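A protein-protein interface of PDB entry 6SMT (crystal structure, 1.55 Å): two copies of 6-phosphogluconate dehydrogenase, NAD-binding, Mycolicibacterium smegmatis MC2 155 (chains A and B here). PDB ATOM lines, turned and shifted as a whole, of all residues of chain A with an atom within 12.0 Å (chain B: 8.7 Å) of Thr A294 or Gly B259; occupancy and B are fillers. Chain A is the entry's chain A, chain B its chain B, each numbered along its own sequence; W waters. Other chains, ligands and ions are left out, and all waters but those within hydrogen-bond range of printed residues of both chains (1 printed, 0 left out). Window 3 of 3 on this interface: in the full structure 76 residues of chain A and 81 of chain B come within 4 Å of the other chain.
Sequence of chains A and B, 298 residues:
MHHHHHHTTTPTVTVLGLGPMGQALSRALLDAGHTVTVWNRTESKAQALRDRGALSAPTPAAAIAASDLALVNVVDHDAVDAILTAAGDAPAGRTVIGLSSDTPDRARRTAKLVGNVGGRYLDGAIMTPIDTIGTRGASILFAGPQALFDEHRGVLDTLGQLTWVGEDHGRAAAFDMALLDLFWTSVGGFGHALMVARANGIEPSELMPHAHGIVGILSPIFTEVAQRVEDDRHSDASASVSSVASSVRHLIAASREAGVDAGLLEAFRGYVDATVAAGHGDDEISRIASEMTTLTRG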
ATOM      1  N   MET A 177       1.860  12.442 -29.384  1.00  0.00           N
ATOM      2  CA  MET A 177       1.775  11.202 -28.533  1.00  0.00           C
ATOM      3  C   MET A 177       3.082  10.407 -28.643  1.00  0.00           C
ATOM      4  O   MET A 177       3.590   9.920 -27.631  1.00  0.00           O
ATOM      5  CB  MET A 177       0.616  10.318 -28.924  1.00  0.00           C
ATOM      6  CG  MET A 177      -0.751  10.950 -28.697  1.00  0.00           C
ATOM      7  SD  MET A 177      -1.216  11.415 -27.009  1.00  0.00           S
ATOM      8  CE  MET A 177      -0.635  13.052 -26.870  1.00  0.00           C
ATOM      9  N   ASP A 181       5.953  10.422 -25.576  1.00  0.00           N
ATOM     10  CA  ASP A 181       6.240   9.085 -25.060  1.00  0.00           C
ATOM     11  C   ASP A 181       7.752   8.940 -24.963  1.00  0.00           C
ATOM     12  O   ASP A 181       8.312   8.618 -23.870  1.00  0.00           O
ATOM     13  CB  ASP A 181       5.612   8.093 -25.986  1.00  0.00           C
ATOM     14  CG  ASP A 181       5.905   6.652 -25.839  1.00  0.00           C
ATOM     15  OD1 ASP A 181       6.477   6.328 -24.712  1.00  0.00           O
ATOM     16  OD2 ASP A 181       5.501   5.877 -26.747  1.00  0.00           O
ATOM     17  N   ALA A 267       9.256  -3.419 -16.735  1.00  0.00           N
ATOM     18  CA  ALA A 267       8.455  -3.478 -17.964  1.00  0.00           C
ATOM     19  C   ALA A 267       9.331  -3.775 -19.143  1.00  0.00           C
ATOM     20  O   ALA A 267       9.050  -4.618 -19.980  1.00  0.00           O
ATOM     21  CB  ALA A 267       7.646  -2.219 -18.082  1.00  0.00           C
ATOM     22  N   GLY A 270      10.400  -7.364 -19.299  1.00  0.00           N
ATOM     23  CA  GLY A 270       9.354  -8.249 -19.817  1.00  0.00           C
ATOM     24  C   GLY A 270       9.391  -8.337 -21.328  1.00  0.00           C
ATOM     25  O   GLY A 270       9.260  -9.427 -21.923  1.00  0.00           O
ATOM     26  N   TYR A 271       9.579  -7.205 -22.013  1.00  0.00           N
ATOM     27  CA  TYR A 271       9.670  -7.254 -23.488  1.00  0.00           C
ATOM     28  C   TYR A 271      10.905  -7.989 -23.944  1.00  0.00           C
ATOM     29  O   TYR A 271      10.879  -8.767 -24.958  1.00  0.00           O
ATOM     30  CB  TYR A 271       9.688  -5.854 -24.096  1.00  0.00           C
ATOM     31  CG  TYR A 271       8.617  -4.962 -23.565  1.00  0.00           C
ATOM     32  CD1 TYR A 271       7.280  -5.361 -23.412  1.00  0.00           C
ATOM     33  CD2 TYR A 271       8.907  -3.640 -23.292  1.00  0.00           C
ATOM     34  CE1 TYR A 271       6.303  -4.481 -22.972  1.00  0.00           C
ATOM     35  CE2 TYR A 271       7.961  -2.759 -22.815  1.00  0.00           C
ATOM     36  CZ  TYR A 271       6.641  -3.176 -22.642  1.00  0.00           C
ATOM     37  OH  TYR A 271       5.658  -2.334 -22.184  1.00  0.00           O
ATOM     38  N   ALA A 274      10.504 -11.715 -23.488  1.00  0.00           N
ATOM     39  CA  ALA A 274       9.541 -12.276 -24.454  1.00  0.00           C
ATOM     40  C   ALA A 274      10.229 -12.406 -25.798  1.00  0.00           C
ATOM     41  O   ALA A 274       9.969 -13.339 -26.547  1.00  0.00           O
ATOM     42  CB  ALA A 274       8.372 -11.427 -24.543  1.00  0.00           C
ATOM     43  N   ILE A 288      13.083  -5.812 -30.034  1.00  0.00           N
ATOM     44  CA  ILE A 288      12.412  -5.912 -28.706  1.00  0.00           C
ATOM     45  C   ILE A 288      11.038  -5.289 -28.816  1.00  0.00           C
ATOM     46  O   ILE A 288      10.081  -5.831 -28.315  1.00  0.00           O
ATOM     47  CB  ILE A 288      13.258  -5.211 -27.620  1.00  0.00           C
ATOM     48  CG1 ILE A 288      14.577  -5.963 -27.398  1.00  0.00           C
ATOM     49  CG2 ILE A 288      12.475  -5.040 -26.337  1.00  0.00           C
ATOM     50  CD1 ILE A 288      15.659  -5.152 -26.690  1.00  0.00           C
ATOM     51  N   ALA A 289      10.907  -4.129 -29.443  1.00  0.00           N
ATOM     52  CA  ALA A 289       9.604  -3.446 -29.450  1.00  0.00           C
ATOM     53  C   ALA A 289       8.504  -4.266 -30.118  1.00  0.00           C
ATOM     54  O   ALA A 289       7.335  -4.025 -29.760  1.00  0.00           O
ATOM     55  CB  ALA A 289       9.675  -2.100 -30.071  1.00  0.00           C
ATOM     56  N   SER A 290       8.829  -5.226 -30.970  1.00  0.00           N
ATOM     57  CA  SER A 290       7.769  -6.125 -31.507  1.00  0.00           C
ATOM     58  C   SER A 290       6.938  -6.699 -30.366  1.00  0.00           C
ATOM     59  O   SER A 290       5.697  -6.844 -30.570  1.00  0.00           O
ATOM     60  CB  SER A 290       8.375  -7.223 -32.329  1.00  0.00           C
ATOM     61  OG  SER A 290       9.031  -6.684 -33.464  1.00  0.00           O
ATOM     62  N   GLU A 291       7.581  -7.079 -29.260  1.00  0.00           N
ATOM     63  CA  GLU A 291       6.928  -7.799 -28.131  1.00  0.00           C
ATOM     64  C   GLU A 291       6.103  -6.832 -27.274  1.00  0.00           C
ATOM     65  O   GLU A 291       5.495  -7.288 -26.302  1.00  0.00           O
ATOM     66  CB  GLU A 291       7.900  -8.636 -27.300  1.00  0.00           C
ATOM     67  CG  GLU A 291       8.526  -9.800 -28.033  1.00  0.00           C
ATOM     68  CD  GLU A 291       7.493 -10.875 -28.387  1.00  0.00           C
ATOM     69  OE1 GLU A 291       6.489 -10.969 -27.662  1.00  0.00           O
ATOM     70  OE2 GLU A 291       7.754 -11.649 -29.311  1.00  0.00           O
ATOM     71  N   MET A 292       6.009  -5.555 -27.654  1.00  0.00           N
ATOM     72  CA  MET A 292       5.181  -4.583 -26.909  1.00  0.00           C
ATOM     73  C   MET A 292       3.718  -4.721 -27.390  1.00  0.00           C
ATOM     74  O   MET A 292       2.870  -4.100 -26.816  1.00  0.00           O
ATOM     75  CB  MET A 292       5.703  -3.153 -27.080  1.00  0.00           C
ATOM     76  CG  MET A 292       7.108  -3.036 -26.496  1.00  0.00           C
ATOM     77  SD  MET A 292       7.705  -1.343 -26.849  1.00  0.00           S
ATOM     78  CE  MET A 292       9.351  -1.312 -26.139  1.00  0.00           C
ATOM     79  N   THR A 293       3.448  -5.436 -28.474  1.00  0.00           N
ATOM     80  CA  THR A 293       1.994  -5.595 -28.865  1.00  0.00           C
ATOM     81  C   THR A 293       1.191  -6.399 -27.822  1.00  0.00           C
ATOM     82  O   THR A 293       1.728  -7.402 -27.296  1.00  0.00           O
ATOM     83  CB  THR A 293       1.826  -6.315 -30.201  1.00  0.00           C
ATOM     84  OG1 THR A 293       2.350  -7.614 -29.933  1.00  0.00           O
ATOM     85  CG2 THR A 293       2.536  -5.590 -31.319  1.00  0.00           C
ATOM     86  N   THR A 294      -0.063  -5.975 -27.544  1.00  0.00           N
ATOM     87  CA  THR A 294      -1.187  -6.763 -26.929  1.00  0.00           C
ATOM     88  C   THR A 294      -2.188  -5.769 -26.323  1.00  0.00           C
ATOM     89  O   THR A 294      -1.696  -4.686 -25.994  1.00  0.00           O
ATOM     90  CB  THR A 294      -0.724  -7.803 -25.889  1.00  0.00           C
ATOM     91  N   HIS B 192       8.825   1.949 -28.216  1.00  0.00           N
ATOM     92  CA  HIS B 192       7.392   2.095 -27.941  1.00  0.00           C
ATOM     93  C   HIS B 192       6.820   3.201 -28.825  1.00  0.00           C
ATOM     94  O   HIS B 192       5.758   3.025 -29.467  1.00  0.00           O
ATOM     95  CB  HIS B 192       7.211   2.334 -26.454  1.00  0.00           C
ATOM     96  CG  HIS B 192       5.804   2.366 -26.053  1.00  0.00           C
ATOM     97  ND1 HIS B 192       5.070   3.517 -26.099  1.00  0.00           N
ATOM     98  CD2 HIS B 192       5.010   1.381 -25.604  1.00  0.00           C
ATOM     99  CE1 HIS B 192       3.819   3.226 -25.646  1.00  0.00           C
ATOM    100  NE2 HIS B 192       3.786   1.937 -25.385  1.00  0.00           N
ATOM    101  N   MET B 195       6.211   2.207 -32.338  1.00  0.00           N
ATOM    102  CA  MET B 195       5.060   1.310 -32.557  1.00  0.00           C
ATOM    103  C   MET B 195       3.784   2.139 -32.505  1.00  0.00           C
ATOM    104  O   MET B 195       2.832   1.879 -33.309  1.00  0.00           O
ATOM    105  CB  MET B 195       5.042   0.222 -31.486  1.00  0.00           C
ATOM    106  CG  MET B 195       6.163  -0.666 -31.574  1.00  0.00           C
ATOM    107  SD  MET B 195       6.073  -1.743 -32.988  1.00  0.00           S
ATOM    108  CE  MET B 195       4.962  -2.891 -32.160  1.00  0.00           C
ATOM    109  N   VAL B 196       3.659   3.094 -31.595  1.00  0.00           N
ATOM    110  CA  VAL B 196       2.417   3.897 -31.477  1.00  0.00           C
ATOM    111  C   VAL B 196       2.351   4.817 -32.692  1.00  0.00           C
ATOM    112  O   VAL B 196       1.243   4.964 -33.272  1.00  0.00           O
ATOM    113  CB  VAL B 196       2.373   4.681 -30.184  1.00  0.00           C
ATOM    114  CG1 VAL B 196       1.144   5.582 -30.179  1.00  0.00           C
ATOM    115  CG2 VAL B 196       2.348   3.727 -29.001  1.00  0.00           C
ATOM    116  N   ALA B 199       1.116   2.811 -35.750  1.00  0.00           N
ATOM    117  CA  ALA B 199      -0.317   2.529 -35.673  1.00  0.00           C
ATOM    118  C   ALA B 199      -1.114   3.764 -36.097  1.00  0.00           C
ATOM    119  O   ALA B 199      -2.316   3.619 -36.514  1.00  0.00           O
ATOM    120  CB  ALA B 199      -0.706   2.076 -34.301  1.00  0.00           C
ATOM    121  N   ASN B 200      -0.590   4.947 -35.911  1.00  0.00           N
ATOM    122  CA  ASN B 200      -1.207   6.245 -36.247  1.00  0.00           C
ATOM    123  C   ASN B 200      -0.816   6.705 -37.653  1.00  0.00           C
ATOM    124  O   ASN B 200      -0.996   7.901 -37.984  1.00  0.00           O
ATOM    125  CB  ASN B 200      -0.897   7.319 -35.198  1.00  0.00           C
ATOM    126  CG  ASN B 200      -1.777   7.192 -33.977  1.00  0.00           C
ATOM    127  OD1 ASN B 200      -2.880   7.775 -33.894  1.00  0.00           O
ATOM    128  ND2 ASN B 200      -1.263   6.492 -32.966  1.00  0.00           N
ATOM    129  N   ILE B 252      -0.824   7.002 -22.314  1.00  0.00           N
ATOM    130  CA  ILE B 252      -1.294   5.622 -22.042  1.00  0.00           C
ATOM    131  C   ILE B 252      -2.574   5.250 -22.846  1.00  0.00           C
ATOM    132  O   ILE B 252      -2.548   4.155 -23.436  1.00  0.00           O
ATOM    133  CB  ILE B 252      -1.497   5.526 -20.551  1.00  0.00           C
ATOM    134  CG1 ILE B 252      -0.161   5.558 -19.816  1.00  0.00           C
ATOM    135  CG2 ILE B 252      -2.271   4.234 -20.237  1.00  0.00           C
ATOM    136  CD1 ILE B 252      -0.253   5.868 -18.334  1.00  0.00           C
ATOM    137  N   ALA B 253      -3.455   6.141 -22.956  1.00  0.00           N
ATOM    138  CA  ALA B 253      -4.671   5.946 -23.802  1.00  0.00           C
ATOM    139  C   ALA B 253      -4.271   5.721 -25.252  1.00  0.00           C
ATOM    140  O   ALA B 253      -4.750   4.797 -25.958  1.00  0.00           O
ATOM    141  CB  ALA B 253      -5.573   7.084 -23.651  1.00  0.00           C
ATOM    142  N   ALA B 254      -3.352   6.540 -25.782  1.00  0.00           N
ATOM    143  CA  ALA B 254      -2.910   6.341 -27.172  1.00  0.00           C
ATOM    144  C   ALA B 254      -2.229   5.025 -27.376  1.00  0.00           C
ATOM    145  O   ALA B 254      -2.376   4.357 -28.460  1.00  0.00           O
ATOM    146  CB  ALA B 254      -2.038   7.532 -27.549  1.00  0.00           C
ATOM    147  N   SER B 255      -1.435   4.528 -26.397  1.00  0.00           N
ATOM    148  CA  SER B 255      -0.751   3.244 -26.511  1.00  0.00           C
ATOM    149  C   SER B 255      -1.832   2.151 -26.630  1.00  0.00           C
ATOM    150  O   SER B 255      -1.706   1.269 -27.478  1.00  0.00           O
ATOM    151  CB  SER B 255       0.199   3.081 -25.357  1.00  0.00           C
ATOM    152  OG  SER B 255       0.896   1.872 -25.402  1.00  0.00           O
ATOM    153  N   ARG B 256      -2.801   2.222 -25.719  1.00  0.00           N
ATOM    154  CA  ARG B 256      -3.922   1.213 -25.609  1.00  0.00           C
ATOM    155  C   ARG B 256      -4.591   1.122 -26.971  1.00  0.00           C
ATOM    156  O   ARG B 256      -4.694  -0.015 -27.540  1.00  0.00           O
ATOM    157  CB  ARG B 256      -4.959   1.614 -24.547  1.00  0.00           C
ATOM    158  CG  ARG B 256      -4.501   1.305 -23.117  1.00  0.00           C
ATOM    159  CD  ARG B 256      -5.501   0.962 -21.987  1.00  0.00           C
ATOM    160  NE  ARG B 256      -5.263   1.756 -20.764  1.00  0.00           N
ATOM    161  CZ  ARG B 256      -6.084   1.796 -19.693  1.00  0.00           C
ATOM    162  NH1 ARG B 256      -7.188   1.042 -19.644  1.00  0.00           N
ATOM    163  NH2 ARG B 256      -5.796   2.583 -18.668  1.00  0.00           N
ATOM    164  N   GLU B 257      -4.940   2.273 -27.493  1.00  0.00           N
ATOM    165  CA  GLU B 257      -5.707   2.378 -28.745  1.00  0.00           C
ATOM    166  C   GLU B 257      -4.900   1.798 -29.896  1.00  0.00           C
ATOM    167  O   GLU B 257      -5.515   1.195 -30.815  1.00  0.00           O
ATOM    168  CB  GLU B 257      -6.127   3.800 -28.989  1.00  0.00           C
ATOM    169  CG  GLU B 257      -6.679   3.935 -30.386  1.00  0.00           C
ATOM    170  CD  GLU B 257      -7.554   5.143 -30.588  1.00  0.00           C
ATOM    171  OE1 GLU B 257      -8.096   5.644 -29.550  1.00  0.00           O
ATOM    172  OE2 GLU B 257      -7.777   5.502 -31.784  1.00  0.00           O
ATOM    173  N   ALA B 258      -3.575   1.920 -29.872  1.00  0.00           N
ATOM    174  CA  ALA B 258      -2.677   1.386 -30.905  1.00  0.00           C
ATOM    175  C   ALA B 258      -2.388  -0.109 -30.740  1.00  0.00           C
ATOM    176  O   ALA B 258      -1.688  -0.703 -31.552  1.00  0.00           O
ATOM    177  CB  ALA B 258      -1.386   2.200 -30.914  1.00  0.00           C
ATOM    178  N   GLY B 259      -2.864  -0.749 -29.688  1.00  0.00           N
ATOM    179  CA  GLY B 259      -2.622  -2.164 -29.441  1.00  0.00           C
ATOM    180  C   GLY B 259      -1.211  -2.370 -28.895  1.00  0.00           C
ATOM    181  O   GLY B 259      -0.639  -3.467 -29.083  1.00  0.00           O
ATOM    182  N   VAL B 260      -0.707  -1.382 -28.142  1.00  0.00           N
ATOM    183  CA  VAL B 260       0.665  -1.496 -27.593  1.00  0.00           C
ATOM    184  C   VAL B 260       0.645  -1.413 -26.057  1.00  0.00           C
ATOM    185  O   VAL B 260      -0.072  -0.553 -25.509  1.00  0.00           O
ATOM    186  CB  VAL B 260       1.533  -0.357 -28.156  1.00  0.00           C
ATOM    187  CG1 VAL B 260       2.963  -0.498 -27.756  1.00  0.00           C
ATOM    188  CG2 VAL B 260       1.431  -0.267 -29.692  1.00  0.00           C
ATOM    189  N   ASP B 261       1.345  -2.323 -25.415  1.00  0.00           N
ATOM    190  CA  ASP B 261       1.459  -2.323 -23.958  1.00  0.00           C
ATOM    191  C   ASP B 261       2.055  -0.978 -23.482  1.00  0.00           C
ATOM    192  O   ASP B 261       2.945  -0.487 -24.167  1.00  0.00           O
ATOM    193  CB  ASP B 261       2.345  -3.460 -23.513  1.00  0.00           C
ATOM    194  CG  ASP B 261       2.444  -3.596 -22.019  1.00  0.00           C
ATOM    195  OD1 ASP B 261       1.418  -4.039 -21.430  1.00  0.00           O
ATOM    196  OD2 ASP B 261       3.426  -3.182 -21.428  1.00  0.00           O
ATOM    197  N   ALA B 262       1.578  -0.433 -22.395  1.00  0.00           N
ATOM    198  CA  ALA B 262       2.051   0.878 -21.893  1.00  0.00           C
ATOM    199  C   ALA B 262       2.754   0.702 -20.541  1.00  0.00           C
ATOM    200  O   ALA B 262       2.709   1.589 -19.736  1.00  0.00           O
ATOM    201  CB  ALA B 262       0.869   1.797 -21.786  1.00  0.00           C
HETATM  202  O   HOH W   1      -0.412  -5.876 -23.162  1.00  0.00           O
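The side-chain carboxylate (OD2) of Asp A181 is in hydrogen-bond range of a ring nitrogen (ND1) of His B192, 2.5 Å away.
The side-chain carboxylate (OD2) of Asp B261 sits at hydrogen-bond distance from the side-chain hydroxyl (OH) of Tyr A271, at 2.5 Å.
The backbone NH of His B192 sits close to the side-chain sulfur of Met A292 (3.7 Å).
The backbone carbonyl oxygen (O) of Met A292 lies within hydrogen-bond range of the backbone NH (N) of Asp B261 (2.7 Å).
The backbone carbonyl oxygen (O) of Gly B259 sits at hydrogen-bond distance from the backbone NH (N) of Thr A294, 3.0 Å away.
OG1 of Thr A293 lies close to O of Ser A290, at 3.5 Å.
NE2 of His B192 sits at hydrogen-bond distance from OG of Ser B255.
A ring nitrogen (NE2) of His B192 lies within hydrogen-bond range of the backbone carbonyl oxygen of Asp B261.
OG of Ser B255 sits at hydrogen-bond distance from O of Val B260, at 2.6 Å.
The side-chain hydroxyl (OG) of Ser B255 is in hydrogen-bond range of the backbone carbonyl oxygen (O) of Asp B261, at 3.4 Å.
Among the printed residues, merely in contact across the chains: Met A177 with Ala B254 (3.8 Å), Ala A289 with Met B195 (3.6 Å), Met A292 with Val B260 (3.5 Å), Thr A293 with Met B195 (3.7 Å), Thr A293 with Gly B259 (3.4 Å) and Thr A294 with Asp B261 (3.9 Å).
Thr A294 touches two residues of chain B.
Gly B259 touches two residues of chain A.
Thr A293 touches just these residues of chain B: Met B195 (3.7 Å) and Gly B259 (3.4 Å).
No residue of chain A comes within 4 Å of Ser B255.
Asp B261 touches just these residues of chain A: Tyr A271, Met A292 and Thr A294.
Of the printed residues of chain B, Asp A181 touches His B192.
Of the printed residues of chain A, Met B195 touches Ala A289 and Thr A293.
Of the printed residues of chain B, Met A292 touches His B192 (3.6 Å), Val B260 (3.5 Å) and Asp B261 (2.7 Å).
Of the printed residues of chain B, Ala A289 touches Met B195 (3.6 Å).
Glu B257 touches none of the printed residues of chain A.
Hydrophobic or aromatic side chains of chain B that line the printed part of chain A: His B192, Met B195, Ala B254 and Val B260.
Of the 13 printed residues of chain A, 7 touch a printed residue of chain B.
Hydrophobic or aromatic side chains of chain A that line the printed part of chain B: Met A177, Tyr A271 and Met A292.
Among the printed residues, no Asp or Glu carboxylate lies within 4 Å of a Lys or Arg side-chain nitrogen of the other chain.
No position is printed for both chains.
Of the 11 pairs that touch across the chains among the printed residues, none has its exchanged pair printed and touching as well.
Water W1 lies within hydrogen-bond range of OD1 of Asp B261 and O of Thr A294.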
